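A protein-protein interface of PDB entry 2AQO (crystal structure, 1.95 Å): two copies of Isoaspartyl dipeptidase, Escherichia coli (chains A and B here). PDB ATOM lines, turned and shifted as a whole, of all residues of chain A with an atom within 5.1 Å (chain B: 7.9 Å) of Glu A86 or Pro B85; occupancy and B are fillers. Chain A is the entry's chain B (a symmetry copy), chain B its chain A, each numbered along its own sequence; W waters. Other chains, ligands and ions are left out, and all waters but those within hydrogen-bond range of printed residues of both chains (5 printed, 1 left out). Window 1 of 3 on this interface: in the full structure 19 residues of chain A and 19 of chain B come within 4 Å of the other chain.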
ATOM      1  N   LEU A  71      33.897 -13.552 -13.761  1.00  0.00           N
ATOM      2  CA  LEU A  71      33.266 -14.390 -14.756  1.00  0.00           C
ATOM      3  C   LEU A  71      31.861 -14.868 -14.449  1.00  0.00           C
ATOM      4  O   LEU A  71      31.043 -14.871 -15.356  1.00  0.00           O
ATOM      5  CB  LEU A  71      34.150 -15.602 -15.167  1.00  0.00           C
ATOM      6  CG  LEU A  71      35.485 -15.213 -15.834  1.00  0.00           C
ATOM      7  CD1 LEU A  71      36.250 -16.505 -16.060  1.00  0.00           C
ATOM      8  CD2 LEU A  71      35.266 -14.531 -17.202  1.00  0.00           C
ATOM      9  N   ILE A  72      31.611 -15.350 -13.214  1.00  0.00           N
ATOM     10  CA  ILE A  72      30.269 -15.885 -12.940  1.00  0.00           C
ATOM     11  C   ILE A  72      29.274 -14.833 -12.457  1.00  0.00           C
ATOM     12  O   ILE A  72      28.098 -15.134 -12.200  1.00  0.00           O
ATOM     13  CB  ILE A  72      30.301 -17.098 -12.004  1.00  0.00           C
ATOM     14  CG1 ILE A  72      31.040 -16.821 -10.690  1.00  0.00           C
ATOM     15  CG2 ILE A  72      30.881 -18.297 -12.764  1.00  0.00           C
ATOM     16  CD1 ILE A  72      30.610 -17.791  -9.559  1.00  0.00           C
ATOM     17  N   GLY A  73      29.779 -13.603 -12.353  1.00  0.00           N
ATOM     18  CA  GLY A  73      29.004 -12.512 -11.816  1.00  0.00           C
ATOM     19  C   GLY A  73      29.677 -12.200 -10.470  1.00  0.00           C
ATOM     20  O   GLY A  73      30.476 -12.983  -9.958  1.00  0.00           O
ATOM     21  N   THR A  84      25.475  -9.495  -9.843  1.00  0.00           N
ATOM     22  CA  THR A  84      25.514  -9.338 -11.300  1.00  0.00           C
ATOM     23  C   THR A  84      25.467 -10.684 -12.037  1.00  0.00           C
ATOM     24  O   THR A  84      25.793 -11.761 -11.520  1.00  0.00           O
ATOM     25  CB  THR A  84      26.705  -8.449 -11.743  1.00  0.00           C
ATOM     26  OG1 THR A  84      27.897  -9.138 -11.402  1.00  0.00           O
ATOM     27  CG2 THR A  84      26.712  -7.123 -10.974  1.00  0.00           C
ATOM     28  N   PRO A  85      25.056 -10.640 -13.301  1.00  0.00           N
ATOM     29  CA  PRO A  85      25.000 -11.853 -14.089  1.00  0.00           C
ATOM     30  C   PRO A  85      26.385 -12.299 -14.629  1.00  0.00           C
ATOM     31  O   PRO A  85      27.399 -11.548 -14.612  1.00  0.00           O
ATOM     32  CB  PRO A  85      24.034 -11.526 -15.232  1.00  0.00           C
ATOM     33  CG  PRO A  85      23.875 -10.009 -15.269  1.00  0.00           C
ATOM     34  CD  PRO A  85      24.557  -9.445 -14.042  1.00  0.00           C
ATOM     35  N   GLU A  86      26.479 -13.549 -15.064  1.00  0.00           N
ATOM     36  CA  GLU A  86      27.737 -14.058 -15.590  1.00  0.00           C
ATOM     37  C   GLU A  86      28.151 -13.287 -16.876  1.00  0.00           C
ATOM     38  O   GLU A  86      27.345 -12.659 -17.561  1.00  0.00           O
ATOM     39  CB  GLU A  86      27.659 -15.576 -15.829  1.00  0.00           C
ATOM     40  CG  GLU A  86      26.689 -15.883 -16.994  1.00  0.00           C
ATOM     41  CD  GLU A  86      26.436 -17.359 -17.216  1.00  0.00           C
ATOM     42  OE1 GLU A  86      27.293 -18.083 -17.658  1.00  0.00           O
ATOM     43  OE2 GLU A  86      25.209 -17.751 -16.968  1.00  0.00           O
ATOM     44  N   VAL A  87      29.419 -13.334 -17.247  1.00  0.00           N
ATOM     45  CA  VAL A  87      29.945 -12.650 -18.424  1.00  0.00           C
ATOM     46  C   VAL A  87      29.640 -13.422 -19.710  1.00  0.00           C
ATOM     47  O   VAL A  87      29.782 -14.652 -19.771  1.00  0.00           O
ATOM     48  CB  VAL A  87      31.485 -12.524 -18.253  1.00  0.00           C
ATOM     49  CG1 VAL A  87      32.130 -11.884 -19.472  1.00  0.00           C
ATOM     50  CG2 VAL A  87      31.729 -11.583 -17.079  1.00  0.00           C
ATOM     51  N   ALA A  88      29.231 -12.726 -20.761  1.00  0.00           N
ATOM     52  CA  ALA A  88      28.999 -13.415 -22.033  1.00  0.00           C
ATOM     53  C   ALA A  88      30.283 -13.341 -22.886  1.00  0.00           C
ATOM     54  O   ALA A  88      31.026 -12.352 -22.845  1.00  0.00           O
ATOM     55  CB  ALA A  88      27.875 -12.744 -22.783  1.00  0.00           C
ATOM     56  N   LYS A 119      32.658 -22.344 -15.361  1.00  0.00           N
ATOM     57  CA  LYS A 119      32.539 -21.244 -16.278  1.00  0.00           C
ATOM     58  C   LYS A 119      33.837 -21.011 -17.031  1.00  0.00           C
ATOM     59  O   LYS A 119      33.879 -20.690 -18.217  1.00  0.00           O
ATOM     60  CB  LYS A 119      32.110 -19.997 -15.532  1.00  0.00           C
ATOM     61  CG  LYS A 119      32.033 -18.780 -16.461  1.00  0.00           C
ATOM     62  CD  LYS A 119      30.825 -18.749 -17.379  1.00  0.00           C
ATOM     63  CE  LYS A 119      30.835 -17.500 -18.245  1.00  0.00           C
ATOM     64  NZ  LYS A 119      29.720 -17.374 -19.209  1.00  0.00           N
ATOM     65  N   ASN A 287      32.635  -6.877 -14.923  1.00  0.00           N
ATOM     66  CA  ASN A 287      31.494  -7.650 -14.439  1.00  0.00           C
ATOM     67  C   ASN A 287      31.182  -7.538 -12.979  1.00  0.00           C
ATOM     68  O   ASN A 287      30.274  -8.200 -12.483  1.00  0.00           O
ATOM     69  CB  ASN A 287      31.518  -9.113 -14.895  1.00  0.00           C
ATOM     70  CG  ASN A 287      30.221  -9.506 -15.542  1.00  0.00           C
ATOM     71  OD1 ASN A 287      29.828  -8.895 -16.554  1.00  0.00           O
ATOM     72  ND2 ASN A 287      29.609 -10.542 -14.958  1.00  0.00           N
ATOM     73  N   PHE A 387      24.538 -19.582 -25.081  1.00  0.00           N
ATOM     74  CA  PHE A 387      23.190 -19.089 -24.783  1.00  0.00           C
ATOM     75  C   PHE A 387      23.049 -17.596 -25.017  1.00  0.00           C
ATOM     76  O   PHE A 387      22.112 -16.953 -24.516  1.00  0.00           O
ATOM     77  CB  PHE A 387      22.766 -19.473 -23.334  1.00  0.00           C
ATOM     78  CG  PHE A 387      22.700 -20.964 -23.174  1.00  0.00           C
ATOM     79  CD1 PHE A 387      23.600 -21.668 -22.363  1.00  0.00           C
ATOM     80  CD2 PHE A 387      21.740 -21.674 -23.895  1.00  0.00           C
ATOM     81  CE1 PHE A 387      23.477 -23.051 -22.267  1.00  0.00           C
ATOM     82  CE2 PHE A 387      21.623 -23.054 -23.827  1.00  0.00           C
ATOM     83  CZ  PHE A 387      22.511 -23.752 -22.990  1.00  0.00           C
ATOM     84  N   HIS B  70      14.140 -23.378 -12.919  1.00  0.00           N
ATOM     85  CA  HIS B  70      15.578 -23.316 -12.623  1.00  0.00           C
ATOM     86  C   HIS B  70      16.090 -21.884 -12.585  1.00  0.00           C
ATOM     87  O   HIS B  70      16.851 -21.441 -13.471  1.00  0.00           O
ATOM     88  CB  HIS B  70      16.408 -24.098 -13.655  1.00  0.00           C
ATOM     89  CG  HIS B  70      15.964 -25.518 -13.566  1.00  0.00           C
ATOM     90  ND1 HIS B  70      16.462 -26.388 -12.607  1.00  0.00           N
ATOM     91  CD2 HIS B  70      15.020 -26.164 -14.282  1.00  0.00           C
ATOM     92  CE1 HIS B  70      15.857 -27.538 -12.793  1.00  0.00           C
ATOM     93  NE2 HIS B  70      15.012 -27.420 -13.786  1.00  0.00           N
ATOM     94  N   LEU B  71      15.631 -21.188 -11.557  1.00  0.00           N
ATOM     95  CA  LEU B  71      15.891 -19.786 -11.313  1.00  0.00           C
ATOM     96  C   LEU B  71      17.357 -19.332 -11.535  1.00  0.00           C
ATOM     97  O   LEU B  71      17.583 -18.240 -12.069  1.00  0.00           O
ATOM     98  CB  LEU B  71      15.483 -19.430  -9.874  1.00  0.00           C
ATOM     99  CG  LEU B  71      13.994 -19.528  -9.614  1.00  0.00           C
ATOM    100  CD1 LEU B  71      13.710 -18.993  -8.218  1.00  0.00           C
ATOM    101  CD2 LEU B  71      13.300 -18.628 -10.637  1.00  0.00           C
ATOM    102  N   ILE B  72      18.360 -20.103 -11.081  1.00  0.00           N
ATOM    103  CA  ILE B  72      19.770 -19.661 -11.234  1.00  0.00           C
ATOM    104  C   ILE B  72      20.433 -20.215 -12.491  1.00  0.00           C
ATOM    105  O   ILE B  72      21.605 -19.953 -12.810  1.00  0.00           O
ATOM    106  CB  ILE B  72      20.641 -19.989  -9.999  1.00  0.00           C
ATOM    107  CG1 ILE B  72      20.879 -21.509  -9.841  1.00  0.00           C
ATOM    108  CG2 ILE B  72      20.107 -19.367  -8.698  1.00  0.00           C
ATOM    109  CD1 ILE B  72      21.829 -21.888  -8.675  1.00  0.00           C
ATOM    110  N   GLY B  73      19.689 -21.026 -13.215  1.00  0.00           N
ATOM    111  CA  GLY B  73      20.214 -21.642 -14.407  1.00  0.00           C
ATOM    112  C   GLY B  73      20.244 -23.140 -14.186  1.00  0.00           C
ATOM    113  O   GLY B  73      20.221 -23.598 -13.044  1.00  0.00           O
ATOM    114  N   GLY B  74      20.280 -23.906 -15.266  1.00  0.00           N
ATOM    115  CA  GLY B  74      20.346 -25.355 -15.161  1.00  0.00           C
ATOM    116  C   GLY B  74      21.320 -25.872 -16.221  1.00  0.00           C
ATOM    117  O   GLY B  74      22.364 -25.262 -16.529  1.00  0.00           O
ATOM    118  N   GLY B  75      20.932 -26.995 -16.795  1.00  0.00           N
ATOM    119  CA  GLY B  75      21.699 -27.635 -17.847  1.00  0.00           C
ATOM    120  C   GLY B  75      23.003 -28.151 -17.311  1.00  0.00           C
ATOM    121  O   GLY B  75      23.104 -28.461 -16.121  1.00  0.00           O
ATOM    122  N   PRO B  80      30.194 -28.106 -19.590  1.00  0.00           N
ATOM    123  CA  PRO B  80      30.072 -26.775 -19.025  1.00  0.00           C
ATOM    124  C   PRO B  80      29.511 -25.723 -19.936  1.00  0.00           C
ATOM    125  O   PRO B  80      28.957 -24.724 -19.438  1.00  0.00           O
ATOM    126  CB  PRO B  80      31.433 -26.386 -18.474  1.00  0.00           C
ATOM    127  CG  PRO B  80      32.370 -27.551 -18.779  1.00  0.00           C
ATOM    128  CD  PRO B  80      31.584 -28.608 -19.541  1.00  0.00           C
ATOM    129  N   THR B  81      29.642 -25.927 -21.263  1.00  0.00           N
ATOM    130  CA  THR B  81      29.058 -24.888 -22.133  1.00  0.00           C
ATOM    131  C   THR B  81      27.496 -24.974 -22.057  1.00  0.00           C
ATOM    132  O   THR B  81      26.784 -24.044 -22.443  1.00  0.00           O
ATOM    133  CB  THR B  81      29.547 -25.024 -23.594  1.00  0.00           C
ATOM    134  OG1 THR B  81      29.058 -26.278 -24.081  1.00  0.00           O
ATOM    135  CG2 THR B  81      31.072 -24.976 -23.678  1.00  0.00           C
ATOM    136  N   THR B  82      26.954 -26.076 -21.512  1.00  0.00           N
ATOM    137  CA  THR B  82      25.504 -26.259 -21.453  1.00  0.00           C
ATOM    138  C   THR B  82      24.799 -25.774 -20.213  1.00  0.00           C
ATOM    139  O   THR B  82      23.625 -26.056 -20.022  1.00  0.00           O
ATOM    140  CB  THR B  82      25.119 -27.684 -21.870  1.00  0.00           C
ATOM    141  OG1 THR B  82      25.551 -28.598 -20.884  1.00  0.00           O
ATOM    142  CG2 THR B  82      25.863 -27.976 -23.179  1.00  0.00           C
ATOM    143  N   ARG B  83      25.524 -25.012 -19.375  1.00  0.00           N
ATOM    144  CA  ARG B  83      24.983 -24.455 -18.154  1.00  0.00           C
ATOM    145  C   ARG B  83      24.144 -23.252 -18.533  1.00  0.00           C
ATOM    146  O   ARG B  83      24.650 -22.270 -19.049  1.00  0.00           O
ATOM    147  CB  ARG B  83      26.092 -24.068 -17.197  1.00  0.00           C
ATOM    148  CG  ARG B  83      26.839 -25.296 -16.706  1.00  0.00           C
ATOM    149  CD  ARG B  83      28.143 -24.970 -15.983  1.00  0.00           C
ATOM    150  NE  ARG B  83      27.936 -24.425 -14.627  1.00  0.00           N
ATOM    151  CZ  ARG B  83      28.027 -23.120 -14.323  1.00  0.00           C
ATOM    152  NH1 ARG B  83      28.292 -22.151 -15.197  1.00  0.00           N
ATOM    153  NH2 ARG B  83      27.787 -22.753 -13.084  1.00  0.00           N
ATOM    154  N   THR B  84      22.862 -23.319 -18.325  1.00  0.00           N
ATOM    155  CA  THR B  84      22.068 -22.175 -18.743  1.00  0.00           C
ATOM    156  C   THR B  84      22.214 -21.050 -17.743  1.00  0.00           C
ATOM    157  O   THR B  84      22.580 -21.206 -16.579  1.00  0.00           O
ATOM    158  CB  THR B  84      20.589 -22.582 -18.935  1.00  0.00           C
ATOM    159  OG1 THR B  84      20.059 -22.889 -17.663  1.00  0.00           O
ATOM    160  CG2 THR B  84      20.523 -23.849 -19.779  1.00  0.00           C
ATOM    161  N   PRO B  85      21.887 -19.882 -18.234  1.00  0.00           N
ATOM    162  CA  PRO B  85      21.969 -18.659 -17.435  1.00  0.00           C
ATOM    163  C   PRO B  85      20.769 -18.498 -16.495  1.00  0.00           C
ATOM    164  O   PRO B  85      19.732 -19.180 -16.622  1.00  0.00           O
ATOM    165  CB  PRO B  85      21.974 -17.533 -18.456  1.00  0.00           C
ATOM    166  CG  PRO B  85      21.605 -18.158 -19.822  1.00  0.00           C
ATOM    167  CD  PRO B  85      21.489 -19.664 -19.648  1.00  0.00           C
ATOM    168  N   GLU B  86      20.909 -17.592 -15.545  1.00  0.00           N
ATOM    169  CA  GLU B  86      19.848 -17.364 -14.594  1.00  0.00           C
ATOM    170  C   GLU B  86      18.605 -16.754 -15.231  1.00  0.00           C
ATOM    171  O   GLU B  86      18.665 -16.137 -16.283  1.00  0.00           O
ATOM    172  CB  GLU B  86      20.380 -16.481 -13.470  1.00  0.00           C
ATOM    173  CG  GLU B  86      20.490 -15.040 -13.996  1.00  0.00           C
ATOM    174  CD  GLU B  86      21.044 -14.087 -12.976  1.00  0.00           C
ATOM    175  OE1 GLU B  86      20.523 -13.920 -11.880  1.00  0.00           O
ATOM    176  OE2 GLU B  86      22.151 -13.504 -13.355  1.00  0.00           O
ATOM    177  N   VAL B  87      17.464 -16.896 -14.567  1.00  0.00           N
ATOM    178  CA  VAL B  87      16.177 -16.340 -15.038  1.00  0.00           C
ATOM    179  C   VAL B  87      16.073 -14.840 -14.776  1.00  0.00           C
ATOM    180  O   VAL B  87      16.438 -14.328 -13.711  1.00  0.00           O
ATOM    181  CB  VAL B  87      14.989 -17.045 -14.367  1.00  0.00           C
ATOM    182  CG1 VAL B  87      13.699 -16.342 -14.735  1.00  0.00           C
ATOM    183  CG2 VAL B  87      14.924 -18.450 -14.939  1.00  0.00           C
ATOM    184  N   ALA B  88      15.542 -14.118 -15.758  1.00  0.00           N
ATOM    185  CA  ALA B  88      15.358 -12.668 -15.635  1.00  0.00           C
ATOM    186  C   ALA B  88      13.921 -12.360 -15.295  1.00  0.00           C
ATOM    187  O   ALA B  88      12.992 -12.960 -15.857  1.00  0.00           O
ATOM    188  CB  ALA B  88      15.738 -11.916 -16.915  1.00  0.00           C
ATOM    189  N   ARG B  91      10.977 -12.102 -17.913  1.00  0.00           N
ATOM    190  CA  ARG B  91      10.583 -13.311 -18.579  1.00  0.00           C
ATOM    191  C   ARG B  91       9.462 -13.976 -17.863  1.00  0.00           C
ATOM    192  O   ARG B  91       8.622 -14.602 -18.484  1.00  0.00           O
ATOM    193  CB  ARG B  91      11.681 -14.365 -18.606  1.00  0.00           C
ATOM    194  CG  ARG B  91      12.822 -13.991 -19.530  1.00  0.00           C
ATOM    195  CD  ARG B  91      12.738 -14.702 -20.874  1.00  0.00           C
ATOM    196  NE  ARG B  91      14.005 -14.528 -21.586  1.00  0.00           N
ATOM    197  CZ  ARG B  91      15.073 -15.354 -21.477  1.00  0.00           C
ATOM    198  NH1 ARG B  91      15.024 -16.434 -20.681  1.00  0.00           N
ATOM    199  NH2 ARG B  91      16.205 -15.084 -22.174  1.00  0.00           N
ATOM    200  N   ARG B 111      26.249 -25.934  -9.035  1.00  0.00           N
ATOM    201  CA  ARG B 111      25.014 -25.239  -8.599  1.00  0.00           C
ATOM    202  C   ARG B 111      24.829 -25.618  -7.139  1.00  0.00           C
ATOM    203  O   ARG B 111      24.932 -26.791  -6.756  1.00  0.00           O
ATOM    204  CB  ARG B 111      23.740 -25.583  -9.364  1.00  0.00           C
ATOM    205  CG  ARG B 111      23.948 -25.622 -10.886  1.00  0.00           C
ATOM    206  CD  ARG B 111      24.142 -24.221 -11.483  1.00  0.00           C
ATOM    207  NE  ARG B 111      23.904 -24.181 -12.953  1.00  0.00           N
ATOM    208  CZ  ARG B 111      23.868 -23.055 -13.677  1.00  0.00           C
ATOM    209  NH1 ARG B 111      24.022 -21.859 -13.121  1.00  0.00           N
ATOM    210  NH2 ARG B 111      23.688 -23.128 -15.019  1.00  0.00           N
ATOM    211  N   LYS B 119      19.012 -15.903  -5.062  1.00  0.00           N
ATOM    212  CA  LYS B 119      18.210 -15.547  -6.241  1.00  0.00           C
ATOM    213  C   LYS B 119      16.729 -15.464  -5.886  1.00  0.00           C
ATOM    214  O   LYS B 119      15.994 -14.576  -6.335  1.00  0.00           O
ATOM    215  CB  LYS B 119      18.460 -16.571  -7.331  1.00  0.00           C
ATOM    216  CG  LYS B 119      17.655 -16.325  -8.606  1.00  0.00           C
ATOM    217  CD  LYS B 119      17.936 -14.982  -9.280  1.00  0.00           C
ATOM    218  CE  LYS B 119      17.213 -14.865 -10.632  1.00  0.00           C
ATOM    219  NZ  LYS B 119      17.746 -13.717 -11.385  1.00  0.00           N
ATOM    220  N   GLY B 286      11.000 -24.319 -16.739  1.00  0.00           N
ATOM    221  CA  GLY B 286      11.636 -23.157 -17.372  1.00  0.00           C
ATOM    222  C   GLY B 286      13.122 -22.984 -16.979  1.00  0.00           C
ATOM    223  O   GLY B 286      13.552 -23.262 -15.849  1.00  0.00           O
ATOM    224  N   ASN B 287      13.897 -22.536 -17.964  1.00  0.00           N
ATOM    225  CA  ASN B 287      15.303 -22.287 -17.793  1.00  0.00           C
ATOM    226  C   ASN B 287      16.171 -23.535 -17.703  1.00  0.00           C
ATOM    227  O   ASN B 287      17.378 -23.491 -17.482  1.00  0.00           O
ATOM    228  CB  ASN B 287      15.585 -21.276 -16.681  1.00  0.00           C
ATOM    229  CG  ASN B 287      16.592 -20.252 -17.102  1.00  0.00           C
ATOM    230  OD1 ASN B 287      16.440 -19.634 -18.166  1.00  0.00           O
ATOM    231  ND2 ASN B 287      17.580 -20.070 -16.213  1.00  0.00           N
ATOM    232  N   GLY B 288      15.524 -24.673 -17.884  1.00  0.00           N
ATOM    233  CA  GLY B 288      16.291 -25.875 -17.921  1.00  0.00           C
ATOM    234  C   GLY B 288      16.857 -25.895 -19.349  1.00  0.00           C
ATOM    235  O   GLY B 288      16.544 -25.053 -20.210  1.00  0.00           O
ATOM    236  N   GLY B 303      18.913 -24.937 -26.707  1.00  0.00           N
ATOM    237  CA  GLY B 303      18.117 -23.829 -26.226  1.00  0.00           C
ATOM    238  C   GLY B 303      17.702 -24.088 -24.798  1.00  0.00           C
ATOM    239  O   GLY B 303      17.876 -25.155 -24.219  1.00  0.00           O
ATOM    240  N   VAL B 304      17.154 -23.062 -24.233  1.00  0.00           N
ATOM    241  CA  VAL B 304      16.718 -23.137 -22.888  1.00  0.00           C
ATOM    242  C   VAL B 304      15.183 -23.018 -22.883  1.00  0.00           C
ATOM    243  O   VAL B 304      14.593 -22.218 -23.642  1.00  0.00           O
ATOM    244  CB  VAL B 304      17.373 -21.932 -22.263  1.00  0.00           C
ATOM    245  CG1 VAL B 304      17.374 -20.824 -23.315  1.00  0.00           C
ATOM    246  CG2 VAL B 304      16.625 -21.497 -21.021  1.00  0.00           C
HETATM  247  O   HOH W   1      25.140 -19.130 -19.565  1.00  0.00           O
HETATM  248  O   HOH W   2      24.555 -20.010 -15.259  1.00  0.00           O
HETATM  249  O   HOH W   3      24.467 -14.143 -11.445  1.00  0.00           O
HETATM  250  O   HOH W   4      27.689 -20.715 -18.786  1.00  0.00           O
HETATM  251  O   HOH W   5      28.150 -19.213 -14.975  1.00  0.00           O
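The side-chain carboxylate (OE1) of Glu A86 is in salt-bridge range of the side-chain amino group (NZ) of Lys A119 (3.0 Å).
OG1 of Thr B84 sits at hydrogen-bond distance from O of Asn B287, 2.8 Å away.
OE1 of Glu B86 lies within salt-bridge range of NZ of Lys B119 (2.8 Å).
The backbone NH of Gly B74 lies within hydrogen-bond range of the side-chain hydroxyl of Thr B84, at 2.6 Å.
The backbone carbonyl oxygen (O) of Thr B84 lies within hydrogen-bond range of the guanidinium group (NH2) of Arg B111.
ND2 of Asn A287 lies within hydrogen-bond range of O of Pro A85.
Among the printed residues, pairs that only touch across the chains: Pro A85 with Glu B86, Glu A86 with Pro B85, Phe A387 with Thr B81, Phe A387 with Arg B83, Phe A387 with Thr B82, Phe A387 with Thr B84 and Phe A387 with Pro B85.
Glu A86 touches just one residue of chain B: Pro B85 (3.4 Å).
Pro B85 touches just these residues of chain A: Glu A86 (3.4 Å) and Phe A387 (3.9 Å).
Printed residues of chain B within 4 Å of Phe A387: Thr B81, Thr B82, Arg B83, Thr B84 and Pro B85.
Of the printed residues of chain A, Thr B84 touches Phe A387 (3.8 Å).
Lys B119 touches none of the printed residues of chain A.
The nearest residue of chain B that does not touch Glu A86 is Thr B84 (4.4 Å).
The nearest printed residue of chain A that does not touch Pro B85 is Pro A85 (7.1 Å).
The nearest printed residue of chain A that does not touch Glu B86 is Thr A84 (4.4 Å).
Of the 23 printed residues of chain B, 6 touch a printed residue of chain A.
Of the 11 printed residues of chain A, 3 touch a printed residue of chain B.
Hydrophobic or aromatic side chains of chain A that line the printed part of chain B: Pro A85 and Phe A387.
Among the printed residues, 7 pairs touch across the chains.
Pro A85 touches Glu B86, and with the chains exchanged Glu A86 touches Pro B85.
Positions printed for both chains: 71, 72, 73, 84, 85, 86, 87, 88, 119 and 287.
Of the 7 pairs that touch across the chains among the printed residues, 2 have their exchanged pair printed and touching as well.
Water W2 lies within hydrogen-bond range of O of Thr B84 (2.7 Å), NH1 of Arg B111 (2.9 Å) and OE2 of Glu A86 (2.9 Å).
Water W3 lies within hydrogen-bond range of O of Thr A84 (2.7 Å) and OE2 of Glu B86 (3.1 Å).
Water W4 lies within hydrogen-bond range of the side-chain carboxylate (OE1) of Glu A86 (2.9 Å) and the backbone carbonyl oxygen (O) of Arg B83 (3.4 Å).
Water W1 bridges OE2 of Glu A86 (2.9 Å) and O of Arg B83 (3.2 Å).
Water W5 bridges the guanidinium group (NH1) of Arg B83 (2.9 Å) and the side-chain carboxylate (OE1) of Glu A86 (3.0 Å).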
